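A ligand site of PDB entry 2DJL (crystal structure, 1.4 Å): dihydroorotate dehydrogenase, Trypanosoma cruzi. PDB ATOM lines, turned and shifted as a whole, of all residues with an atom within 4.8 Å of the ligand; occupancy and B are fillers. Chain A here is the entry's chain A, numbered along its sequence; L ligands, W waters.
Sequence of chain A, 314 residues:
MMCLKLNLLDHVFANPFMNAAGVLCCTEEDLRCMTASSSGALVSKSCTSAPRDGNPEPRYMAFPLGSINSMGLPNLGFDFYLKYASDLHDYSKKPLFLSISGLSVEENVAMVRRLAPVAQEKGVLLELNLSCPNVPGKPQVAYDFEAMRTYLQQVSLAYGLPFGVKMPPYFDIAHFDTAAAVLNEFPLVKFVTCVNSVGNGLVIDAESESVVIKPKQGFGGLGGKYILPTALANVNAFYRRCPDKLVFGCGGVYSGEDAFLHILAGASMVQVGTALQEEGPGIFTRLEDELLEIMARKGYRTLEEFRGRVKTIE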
ATOM      1  N   ALA A  20      15.230  -1.501  22.004  1.00  0.00           N
ATOM      2  CA  ALA A  20      13.980  -2.165  21.690  1.00  0.00           C
ATOM      3  C   ALA A  20      13.309  -1.375  20.573  1.00  0.00           C
ATOM      4  O   ALA A  20      13.387  -0.136  20.534  1.00  0.00           O
ATOM      5  CB  ALA A  20      13.104  -2.210  22.914  1.00  0.00           C
ATOM      6  N   ALA A  21      12.644  -2.063  19.645  1.00  0.00           N
ATOM      7  CA  ALA A  21      11.978  -1.372  18.562  1.00  0.00           C
ATOM      8  C   ALA A  21      11.040  -0.293  19.083  1.00  0.00           C
ATOM      9  O   ALA A  21      10.341  -0.481  20.103  1.00  0.00           O
ATOM     10  CB  ALA A  21      11.219  -2.352  17.681  1.00  0.00           C
ATOM     11  N   GLY A  22      11.038   0.842  18.398  1.00  0.00           N
ATOM     12  CA  GLY A  22      10.209   1.977  18.800  1.00  0.00           C
ATOM     13  C   GLY A  22      10.905   3.021  19.646  1.00  0.00           C
ATOM     14  O   GLY A  22      10.463   4.161  19.690  1.00  0.00           O
ATOM     15  N   VAL A  23      11.988   2.645  20.331  1.00  0.00           N
ATOM     16  CA  VAL A  23      12.701   3.580  21.194  1.00  0.00           C
ATOM     17  C   VAL A  23      13.963   4.069  20.483  1.00  0.00           C
ATOM     18  O   VAL A  23      14.786   3.268  20.047  1.00  0.00           O
ATOM     19  CB  VAL A  23      13.035   2.939  22.561  1.00  0.00           C
ATOM     20  CG1 VAL A  23      13.826   3.918  23.416  1.00  0.00           C
ATOM     21  CG2 VAL A  23      11.752   2.529  23.283  1.00  0.00           C
ATOM     22  N   LYS A  45      12.193   1.795  14.052  1.00  0.00           N
ATOM     23  CA  LYS A  45      10.807   1.887  14.478  1.00  0.00           C
ATOM     24  C   LYS A  45       9.922   0.994  13.607  1.00  0.00           C
ATOM     25  O   LYS A  45      10.052   1.002  12.379  1.00  0.00           O
ATOM     26  CB  LYS A  45      10.341   3.345  14.364  1.00  0.00           C
ATOM     27  CG  LYS A  45       8.827   3.564  14.492  1.00  0.00           C
ATOM     28  CD  LYS A  45       8.345   3.314  15.914  1.00  0.00           C
ATOM     29  CE  LYS A  45       6.831   3.189  16.012  1.00  0.00           C
ATOM     30  NZ  LYS A  45       6.401   2.881  17.427  1.00  0.00           N
ATOM     31  N   SER A  46       9.015   0.240  14.231  1.00  0.00           N
ATOM     32  CA  SER A  46       8.067  -0.559  13.455  1.00  0.00           C
ATOM     33  C   SER A  46       7.352   0.326  12.445  1.00  0.00           C
ATOM     34  O   SER A  46       6.767   1.357  12.802  1.00  0.00           O
ATOM     35  CB  SER A  46       7.036  -1.233  14.339  1.00  0.00           C
ATOM     36  OG  SER A  46       7.618  -2.300  15.057  1.00  0.00           O
ATOM     37  N   TYR A  60       2.781   8.783  25.769  1.00  0.00           N
ATOM     38  CA  TYR A  60       3.835   8.081  26.507  1.00  0.00           C
ATOM     39  C   TYR A  60       4.006   8.754  27.855  1.00  0.00           C
ATOM     40  O   TYR A  60       4.075   9.974  27.931  1.00  0.00           O
ATOM     41  CB  TYR A  60       5.171   8.116  25.754  1.00  0.00           C
ATOM     42  CG  TYR A  60       6.315   7.568  26.581  1.00  0.00           C
ATOM     43  CD1 TYR A  60       7.113   8.409  27.365  1.00  0.00           C
ATOM     44  CD2 TYR A  60       6.612   6.203  26.568  1.00  0.00           C
ATOM     45  CE1 TYR A  60       8.155   7.885  28.146  1.00  0.00           C
ATOM     46  CE2 TYR A  60       7.650   5.674  27.325  1.00  0.00           C
ATOM     47  CZ  TYR A  60       8.419   6.517  28.100  1.00  0.00           C
ATOM     48  OH  TYR A  60       9.451   5.990  28.845  1.00  0.00           O
ATOM     49  N   SER A  67       6.896   2.309  32.216  1.00  0.00           N
ATOM     50  CA  SER A  67       6.213   3.223  31.310  1.00  0.00           C
ATOM     51  C   SER A  67       4.912   2.658  30.783  1.00  0.00           C
ATOM     52  O   SER A  67       4.686   1.442  30.783  1.00  0.00           O
ATOM     53  CB  SER A  67       7.132   3.578  30.126  1.00  0.00           C
ATOM     54  OG  SER A  67       7.313   2.461  29.274  1.00  0.00           O
ATOM     55  N   ASN A  69       2.425   3.371  27.220  1.00  0.00           N
ATOM     56  CA  ASN A  69       2.330   4.092  25.963  1.00  0.00           C
ATOM     57  C   ASN A  69       1.207   3.599  25.098  1.00  0.00           C
ATOM     58  O   ASN A  69       0.831   2.429  25.146  1.00  0.00           O
ATOM     59  CB  ASN A  69       3.658   4.029  25.177  1.00  0.00           C
ATOM     60  CG  ASN A  69       3.738   2.819  24.253  1.00  0.00           C
ATOM     61  OD1 ASN A  69       3.230   2.842  23.121  1.00  0.00           O
ATOM     62  ND2 ASN A  69       4.380   1.749  24.727  1.00  0.00           N
ATOM     63  N   MET A  71       1.466   4.666  21.443  1.00  0.00           N
ATOM     64  CA  MET A  71       2.012   5.476  20.354  1.00  0.00           C
ATOM     65  C   MET A  71       1.150   5.415  19.098  1.00  0.00           C
ATOM     66  O   MET A  71       0.864   6.450  18.478  1.00  0.00           O
ATOM     67  CB  MET A  71       3.456   5.074  20.022  1.00  0.00           C
ATOM     68  CG  MET A  71       4.438   5.135  21.199  1.00  0.00           C
ATOM     69  SD  MET A  71       4.526   6.727  22.063  1.00  0.00           S
ATOM     70  CE  MET A  71       5.365   7.726  20.827  1.00  0.00           C
ATOM     71  N   LEU A  73       1.889   3.406  16.290  1.00  0.00           N
ATOM     72  CA  LEU A  73       2.771   3.247  15.126  1.00  0.00           C
ATOM     73  C   LEU A  73       3.054   4.548  14.350  1.00  0.00           C
ATOM     74  O   LEU A  73       3.017   4.553  13.119  1.00  0.00           O
ATOM     75  CB  LEU A  73       2.278   2.143  14.185  1.00  0.00           C
ATOM     76  CG  LEU A  73       2.316   0.718  14.734  1.00  0.00           C
ATOM     77  CD1 LEU A  73       1.626  -0.233  13.774  1.00  0.00           C
ATOM     78  CD2 LEU A  73       3.751   0.242  15.009  1.00  0.00           C
ATOM     79  N   SER A  99      12.263  -3.250  11.665  1.00  0.00           N
ATOM     80  CA  SER A  99      11.011  -3.775  12.185  1.00  0.00           C
ATOM     81  C   SER A  99       9.857  -3.338  11.308  1.00  0.00           C
ATOM     82  O   SER A  99       9.729  -2.165  10.982  1.00  0.00           O
ATOM     83  CB  SER A  99      10.778  -3.323  13.627  1.00  0.00           C
ATOM     84  OG  SER A  99       9.495  -3.739  14.065  1.00  0.00           O
ATOM     85  N   GLU A 127      12.760  -7.909  11.602  1.00  0.00           N
ATOM     86  CA  GLU A 127      11.973  -8.264  12.789  1.00  0.00           C
ATOM     87  C   GLU A 127      10.503  -7.961  12.489  1.00  0.00           C
ATOM     88  O   GLU A 127      10.115  -6.805  12.354  1.00  0.00           O
ATOM     89  CB  GLU A 127      12.441  -7.502  14.039  1.00  0.00           C
ATOM     90  CG  GLU A 127      11.753  -7.979  15.328  1.00  0.00           C
ATOM     91  CD  GLU A 127      12.277  -7.299  16.588  1.00  0.00           C
ATOM     92  OE1 GLU A 127      11.794  -6.193  16.923  1.00  0.00           O
ATOM     93  OE2 GLU A 127      13.163  -7.875  17.246  1.00  0.00           O
ATOM     94  N   ASN A 129       6.791  -7.595  13.457  1.00  0.00           N
ATOM     95  CA  ASN A 129       6.078  -7.297  14.690  1.00  0.00           C
ATOM     96  C   ASN A 129       4.668  -7.873  14.673  1.00  0.00           C
ATOM     97  O   ASN A 129       3.809  -7.397  13.941  1.00  0.00           O
ATOM     98  CB  ASN A 129       6.049  -5.777  14.912  1.00  0.00           C
ATOM     99  CG  ASN A 129       5.423  -5.368  16.227  1.00  0.00           C
ATOM    100  OD1 ASN A 129       4.970  -6.194  17.011  1.00  0.00           O
ATOM    101  ND2 ASN A 129       5.415  -4.069  16.481  1.00  0.00           N
ATOM    102  N   LYS A 166       8.678 -10.444  16.655  1.00  0.00           N
ATOM    103  CA  LYS A 166       8.465  -9.790  17.941  1.00  0.00           C
ATOM    104  C   LYS A 166       7.147 -10.294  18.541  1.00  0.00           C
ATOM    105  O   LYS A 166       6.061 -10.057  17.992  1.00  0.00           O
ATOM    106  CB  LYS A 166       8.445  -8.265  17.769  1.00  0.00           C
ATOM    107  CG  LYS A 166       8.278  -7.449  19.064  1.00  0.00           C
ATOM    108  CD  LYS A 166       9.540  -7.481  19.928  1.00  0.00           C
ATOM    109  CE  LYS A 166       9.455  -6.481  21.079  1.00  0.00           C
ATOM    110  NZ  LYS A 166       9.592  -5.066  20.615  1.00  0.00           N
ATOM    111  N   VAL A 195       9.963  -9.783  25.098  1.00  0.00           N
ATOM    112  CA  VAL A 195       8.572  -9.592  24.677  1.00  0.00           C
ATOM    113  C   VAL A 195       8.324  -8.129  24.262  1.00  0.00           C
ATOM    114  O   VAL A 195       9.075  -7.222  24.629  1.00  0.00           O
ATOM    115  CB  VAL A 195       7.580  -9.910  25.841  1.00  0.00           C
ATOM    116  CG1 VAL A 195       7.612 -11.380  26.173  1.00  0.00           C
ATOM    117  CG2 VAL A 195       7.865  -9.066  27.107  1.00  0.00           C
ATOM    118  N   ASN A 196       7.243  -7.934  23.515  1.00  0.00           N
ATOM    119  CA  ASN A 196       6.605  -6.625  23.373  1.00  0.00           C
ATOM    120  C   ASN A 196       5.944  -6.221  24.690  1.00  0.00           C
ATOM    121  O   ASN A 196       5.952  -6.991  25.673  1.00  0.00           O
ATOM    122  CB  ASN A 196       5.590  -6.686  22.238  1.00  0.00           C
ATOM    123  CG  ASN A 196       5.474  -5.373  21.464  1.00  0.00           C
ATOM    124  OD1 ASN A 196       5.428  -4.288  22.052  1.00  0.00           O
ATOM    125  ND2 ASN A 196       5.414  -5.468  20.135  1.00  0.00           N
ATOM    126  N   SER A 197       5.371  -5.021  24.726  1.00  0.00           N
ATOM    127  CA  SER A 197       4.735  -4.523  25.943  1.00  0.00           C
ATOM    128  C   SER A 197       3.690  -5.464  26.513  1.00  0.00           C
ATOM    129  O   SER A 197       3.005  -6.185  25.768  1.00  0.00           O
ATOM    130  CB  SER A 197       4.060  -3.182  25.681  1.00  0.00           C
ATOM    131  OG  SER A 197       4.935  -2.271  25.057  1.00  0.00           O
ATOM    132  N   GLY A 223       5.809  -1.259  30.003  1.00  0.00           N
ATOM    133  CA  GLY A 223       7.199  -1.697  29.960  1.00  0.00           C
ATOM    134  C   GLY A 223       7.909  -1.299  31.235  1.00  0.00           C
ATOM    135  O   GLY A 223       7.340  -0.602  32.092  1.00  0.00           O
ATOM    136  N   GLY A 224       9.151  -1.765  31.378  1.00  0.00           N
ATOM    137  CA  GLY A 224       9.987  -1.395  32.516  1.00  0.00           C
ATOM    138  C   GLY A 224       9.950  -2.390  33.664  1.00  0.00           C
ATOM    139  O   GLY A 224       9.762  -3.590  33.436  1.00  0.00           O
ATOM    140  N   ILE A 227       7.497  -5.403  34.242  1.00  0.00           N
ATOM    141  CA  ILE A 227       7.360  -6.545  33.341  1.00  0.00           C
ATOM    142  C   ILE A 227       8.528  -7.526  33.337  1.00  0.00           C
ATOM    143  O   ILE A 227       8.508  -8.503  32.586  1.00  0.00           O
ATOM    144  CB  ILE A 227       6.994  -6.110  31.885  1.00  0.00           C
ATOM    145  CG1 ILE A 227       8.207  -5.625  31.093  1.00  0.00           C
ATOM    146  CG2 ILE A 227       5.868  -5.068  31.896  1.00  0.00           C
ATOM    147  CD1 ILE A 227       7.962  -5.628  29.588  1.00  0.00           C
ATOM    148  N   CYS A 250      13.678  -8.994  25.754  1.00  0.00           N
ATOM    149  CA  CYS A 250      13.270  -7.602  25.849  1.00  0.00           C
ATOM    150  C   CYS A 250      12.258  -7.492  26.974  1.00  0.00           C
ATOM    151  O   CYS A 250      11.316  -8.280  27.041  1.00  0.00           O
ATOM    152  CB  CYS A 250      12.638  -7.144  24.537  1.00  0.00           C
ATOM    153  SG  CYS A 250      12.267  -5.377  24.470  1.00  0.00           S
ATOM    154  N   GLY A 251      12.473  -6.542  27.868  1.00  0.00           N
ATOM    155  CA  GLY A 251      11.507  -6.294  28.931  1.00  0.00           C
ATOM    156  C   GLY A 251      12.171  -6.130  30.272  1.00  0.00           C
ATOM    157  O   GLY A 251      12.778  -7.062  30.809  1.00  0.00           O
ATOM    158  N   GLY A 252      12.071  -4.924  30.816  1.00  0.00           N
ATOM    159  CA  GLY A 252      12.534  -4.666  32.176  1.00  0.00           C
ATOM    160  C   GLY A 252      14.031  -4.567  32.390  1.00  0.00           C
ATOM    161  O   GLY A 252      14.496  -4.681  33.527  1.00  0.00           O
ATOM    162  N   VAL A 253      14.807  -4.340  31.321  1.00  0.00           N
ATOM    163  CA  VAL A 253      16.262  -4.219  31.472  1.00  0.00           C
ATOM    164  C   VAL A 253      16.673  -2.803  31.847  1.00  0.00           C
ATOM    165  O   VAL A 253      16.488  -1.874  31.038  1.00  0.00           O
ATOM    166  CB  VAL A 253      17.010  -4.672  30.205  1.00  0.00           C
ATOM    167  CG1 VAL A 253      18.530  -4.451  30.342  1.00  0.00           C
ATOM    168  CG2 VAL A 253      16.712  -6.132  29.900  1.00  0.00           C
ATOM    169  N   GLN A 271      17.444  -6.468  24.408  1.00  0.00           N
ATOM    170  CA  GLN A 271      16.922  -5.183  23.964  1.00  0.00           C
ATOM    171  C   GLN A 271      16.487  -4.328  25.148  1.00  0.00           C
ATOM    172  O   GLN A 271      16.030  -4.843  26.178  1.00  0.00           O
ATOM    173  CB  GLN A 271      15.748  -5.379  23.024  1.00  0.00           C
ATOM    174  CG  GLN A 271      15.995  -6.405  21.920  1.00  0.00           C
ATOM    175  CD  GLN A 271      14.888  -6.416  20.892  1.00  0.00           C
ATOM    176  OE1 GLN A 271      13.737  -6.052  21.176  1.00  0.00           O
ATOM    177  NE2 GLN A 271      15.212  -6.840  19.676  1.00  0.00           N
ATOM    178  N   VAL A 272      16.628  -3.012  24.978  1.00  0.00           N
ATOM    179  CA  VAL A 272      16.371  -2.047  26.051  1.00  0.00           C
ATOM    180  C   VAL A 272      15.396  -0.983  25.557  1.00  0.00           C
ATOM    181  O   VAL A 272      15.694  -0.251  24.607  1.00  0.00           O
ATOM    182  CB  VAL A 272      17.695  -1.389  26.496  1.00  0.00           C
ATOM    183  CG1 VAL A 272      17.466  -0.529  27.727  1.00  0.00           C
ATOM    184  CG2 VAL A 272      18.767  -2.476  26.780  1.00  0.00           C
ATOM    185  N   GLY A 273      14.225  -0.920  26.203  1.00  0.00           N
ATOM    186  CA  GLY A 273      13.172  -0.001  25.801  1.00  0.00           C
ATOM    187  C   GLY A 273      13.026   1.159  26.758  1.00  0.00           C
ATOM    188  O   GLY A 273      13.706   2.180  26.625  1.00  0.00           O
ATOM    189  N   THR A 274      12.128   1.001  27.727  1.00  0.00           N
ATOM    190  CA  THR A 274      11.837   2.046  28.728  1.00  0.00           C
ATOM    191  C   THR A 274      13.092   2.671  29.333  1.00  0.00           C
ATOM    192  O   THR A 274      13.183   3.893  29.405  1.00  0.00           O
ATOM    193  CB  THR A 274      10.909   1.499  29.837  1.00  0.00           C
ATOM    194  OG1 THR A 274       9.670   1.097  29.262  1.00  0.00           O
ATOM    195  CG2 THR A 274      10.645   2.555  30.899  1.00  0.00           C
ATOM    196  N   ALA A 275      14.041   1.853  29.777  1.00  0.00           N
ATOM    197  CA  ALA A 275      15.233   2.413  30.425  1.00  0.00           C
ATOM    198  C   ALA A 275      16.039   3.288  29.473  1.00  0.00           C
ATOM    199  O   ALA A 275      16.618   4.300  29.887  1.00  0.00           O
ATOM    200  CB  ALA A 275      16.080   1.314  31.021  1.00  0.00           C
HETATM  201  N1  LIG L   1       7.810  -2.567  20.019  1.00  0.00           N
HETATM  202  C1  LIG L   1       7.799  -2.889  18.691  1.00  0.00           C
HETATM  203  O1  LIG L   1       7.942  -4.067  18.350  1.00  0.00           O
HETATM  204  N2  LIG L   1       7.630  -1.898  17.741  1.00  0.00           N
HETATM  205  C2  LIG L   1       7.488  -0.572  18.079  1.00  0.00           C
HETATM  206  O2  LIG L   1       7.542   0.293  17.180  1.00  0.00           O
HETATM  207  C3  LIG L   1       7.510  -0.239  19.420  1.00  0.00           C
HETATM  208  N3  LIG L   1       7.371   1.075  19.811  1.00  0.00           N
HETATM  209  C4  LIG L   1       7.448   1.392  21.152  1.00  0.00           C
HETATM  210  C5  LIG L   1       7.327   2.715  21.568  1.00  0.00           C
HETATM  211  C6  LIG L   1       7.394   3.064  22.920  1.00  0.00           C
HETATM  212  C7  LIG L   1       7.610   4.516  23.250  1.00  0.00           C
HETATM  213  C8  LIG L   1       7.581   2.060  23.867  1.00  0.00           C
HETATM  214  C9  LIG L   1       8.012   2.390  25.283  1.00  0.00           C
HETATM  215  C10 LIG L   1       7.673   0.731  23.464  1.00  0.00           C
HETATM  216  C11 LIG L   1       7.625   0.391  22.120  1.00  0.00           C
HETATM  217  N4  LIG L   1       7.730  -0.936  21.720  1.00  0.00           N
HETATM  218  C12 LIG L   1       7.686  -1.241  20.389  1.00  0.00           C
HETATM  219  C13 LIG L   1       7.827  -2.041  22.718  1.00  0.00           C
HETATM  220  C14 LIG L   1       9.303  -2.195  23.086  1.00  0.00           C
HETATM  221  O3  LIG L   1      10.045  -2.603  21.953  1.00  0.00           O
HETATM  222  C15 LIG L   1       9.491  -3.244  24.177  1.00  0.00           C
HETATM  223  O4  LIG L   1       9.013  -4.480  23.689  1.00  0.00           O
HETATM  224  C16 LIG L   1       8.763  -2.886  25.479  1.00  0.00           C
HETATM  225  O5  LIG L   1       8.878  -1.497  25.744  1.00  0.00           O
HETATM  226  C17 LIG L   1       9.261  -3.697  26.675  1.00  0.00           C
HETATM  227  O6  LIG L   1      10.630  -3.454  26.929  1.00  0.00           O
HETATM  228  P1  LIG L   1      11.045  -2.460  28.149  1.00  0.00           P
HETATM  229  O7  LIG L   1      10.544  -3.072  29.433  1.00  0.00           O
HETATM  230  O8  LIG L   1      12.557  -2.351  28.097  1.00  0.00           O
HETATM  231  O9  LIG L   1      10.365  -1.133  27.886  1.00  0.00           O
HETATM  232  O   HOH W   1      14.281  -4.438  28.312  1.00  0.00           O
HETATM  233  O   HOH W   2       9.408  -5.265  16.178  1.00  0.00           O
HETATM  234  O   HOH W   3      13.899  -0.969  30.013  1.00  0.00           O
HETATM  235  O   HOH W   4       6.403  -0.943  26.764  1.00  0.00           O
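The backbone NH (N) of Thr 274 lies within hydrogen-bond range of an oxygen (O9) of the ligand.
The side-chain hydroxyl of Thr 274 is in hydrogen-bond range of an oxygen (O9) of the ligand (2.7 Å).
An oxygen (O2) of the ligand lies close to the backbone NH (N) of Ser 46, 3.3 Å away.
The side-chain hydroxyl (OG) of Ser 46 is in hydrogen-bond range of a nitrogen (N2) of the ligand (2.7 Å).
The backbone NH (N) of Gly 224 is in hydrogen-bond range of an oxygen (O7) of the ligand (2.7 Å).
The backbone NH (N) of Gly 252 sits at hydrogen-bond distance from an oxygen (O7) of the ligand.
O of Ala 21 sits close to O3 of the ligand.
The side-chain amino group of Lys 45 lies within hydrogen-bond range of an oxygen (O2) of the ligand.
An oxygen (O3) of the ligand lies within hydrogen-bond range of the side-chain amino group (NZ) of Lys 166, 2.8 Å away.
O of Val 195 is in hydrogen-bond range of O4 of the ligand (2.9 Å).
N of Gly 273 is in hydrogen-bond range of O8 of the ligand.
An oxygen (O1) of the ligand sits at hydrogen-bond distance from the side-chain amide nitrogen of Asn 129 (3.1 Å).
An oxygen (O1) of the ligand sits at hydrogen-bond distance from the side-chain amide nitrogen (ND2) of Asn 196 (3.4 Å).
SG of Cys 250 lies within hydrogen-bond range of O4 of the ligand, 3.5 Å away.
The side-chain hydroxyl (OG1) of Thr 274 is in hydrogen-bond range of the side-chain hydroxyl (OG) of Ser 67, 2.7 Å away.
OG of Ser 46 lies within hydrogen-bond range of ND2 of Asn 129.
OG of Ser 99 sits at hydrogen-bond distance from OG of Ser 46 (2.6 Å).
The side-chain amide oxygen (OD1) of Asn 129 lies within hydrogen-bond range of the side-chain amide nitrogen (ND2) of Asn 196 (3.2 Å).
N of Ala 20 sits at hydrogen-bond distance from O of Val 272 (2.9 Å).
The side-chain amide oxygen of Asn 69 lies within hydrogen-bond range of the backbone NH of Met 71 (3.0 Å).
The side-chain amide oxygen of Gln 271 is in hydrogen-bond range of the side-chain sulfur of Cys 250 (3.7 Å).
The backbone carbonyl oxygen (O) of Gly 223 lies within hydrogen-bond range of the backbone NH (N) of Ser 67.
Residues that only touch the ligand: Ala 20 (3.2 Å), Gly 22 (3.1 Å), Tyr 60 (3.9 Å), Asn 69 (3.3 Å), Met 71 (3.8 Å), Ser 197 (3.7 Å), Gly 223 (3.7 Å), Ile 227 (3.6 Å) and Gly 251 (3.4 Å).
Within 4 Å of the ligand: Ala 20, Ala 21, Gly 22, Lys 45, Ser 46, Tyr 60, Asn 69, Met 71, Asn 129, Lys 166, Val 195, Asn 196, Ser 197, Gly 223, Gly 224, Ile 227, Cys 250, Gly 251, Gly 252, Gly 273 and Thr 274.
Water W3 lies within hydrogen-bond range of an oxygen (O8) of the ligand (2.7 Å), the backbone NH (N) of Ala 275 (2.8 Å), the backbone carbonyl oxygen (O) of Val 253 (2.9 Å) and the backbone NH (N) of Thr 274 (3.5 Å).
Water W4 lies within hydrogen-bond range of the side-chain hydroxyl of Ser 197 (2.6 Å), an oxygen (O5) of the ligand (2.7 Å) and the backbone NH of Gly 223 (3.3 Å).
Water W2 lies within hydrogen-bond range of OG of Ser 99, OE1 of Glu 127 and O1 of the ligand.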
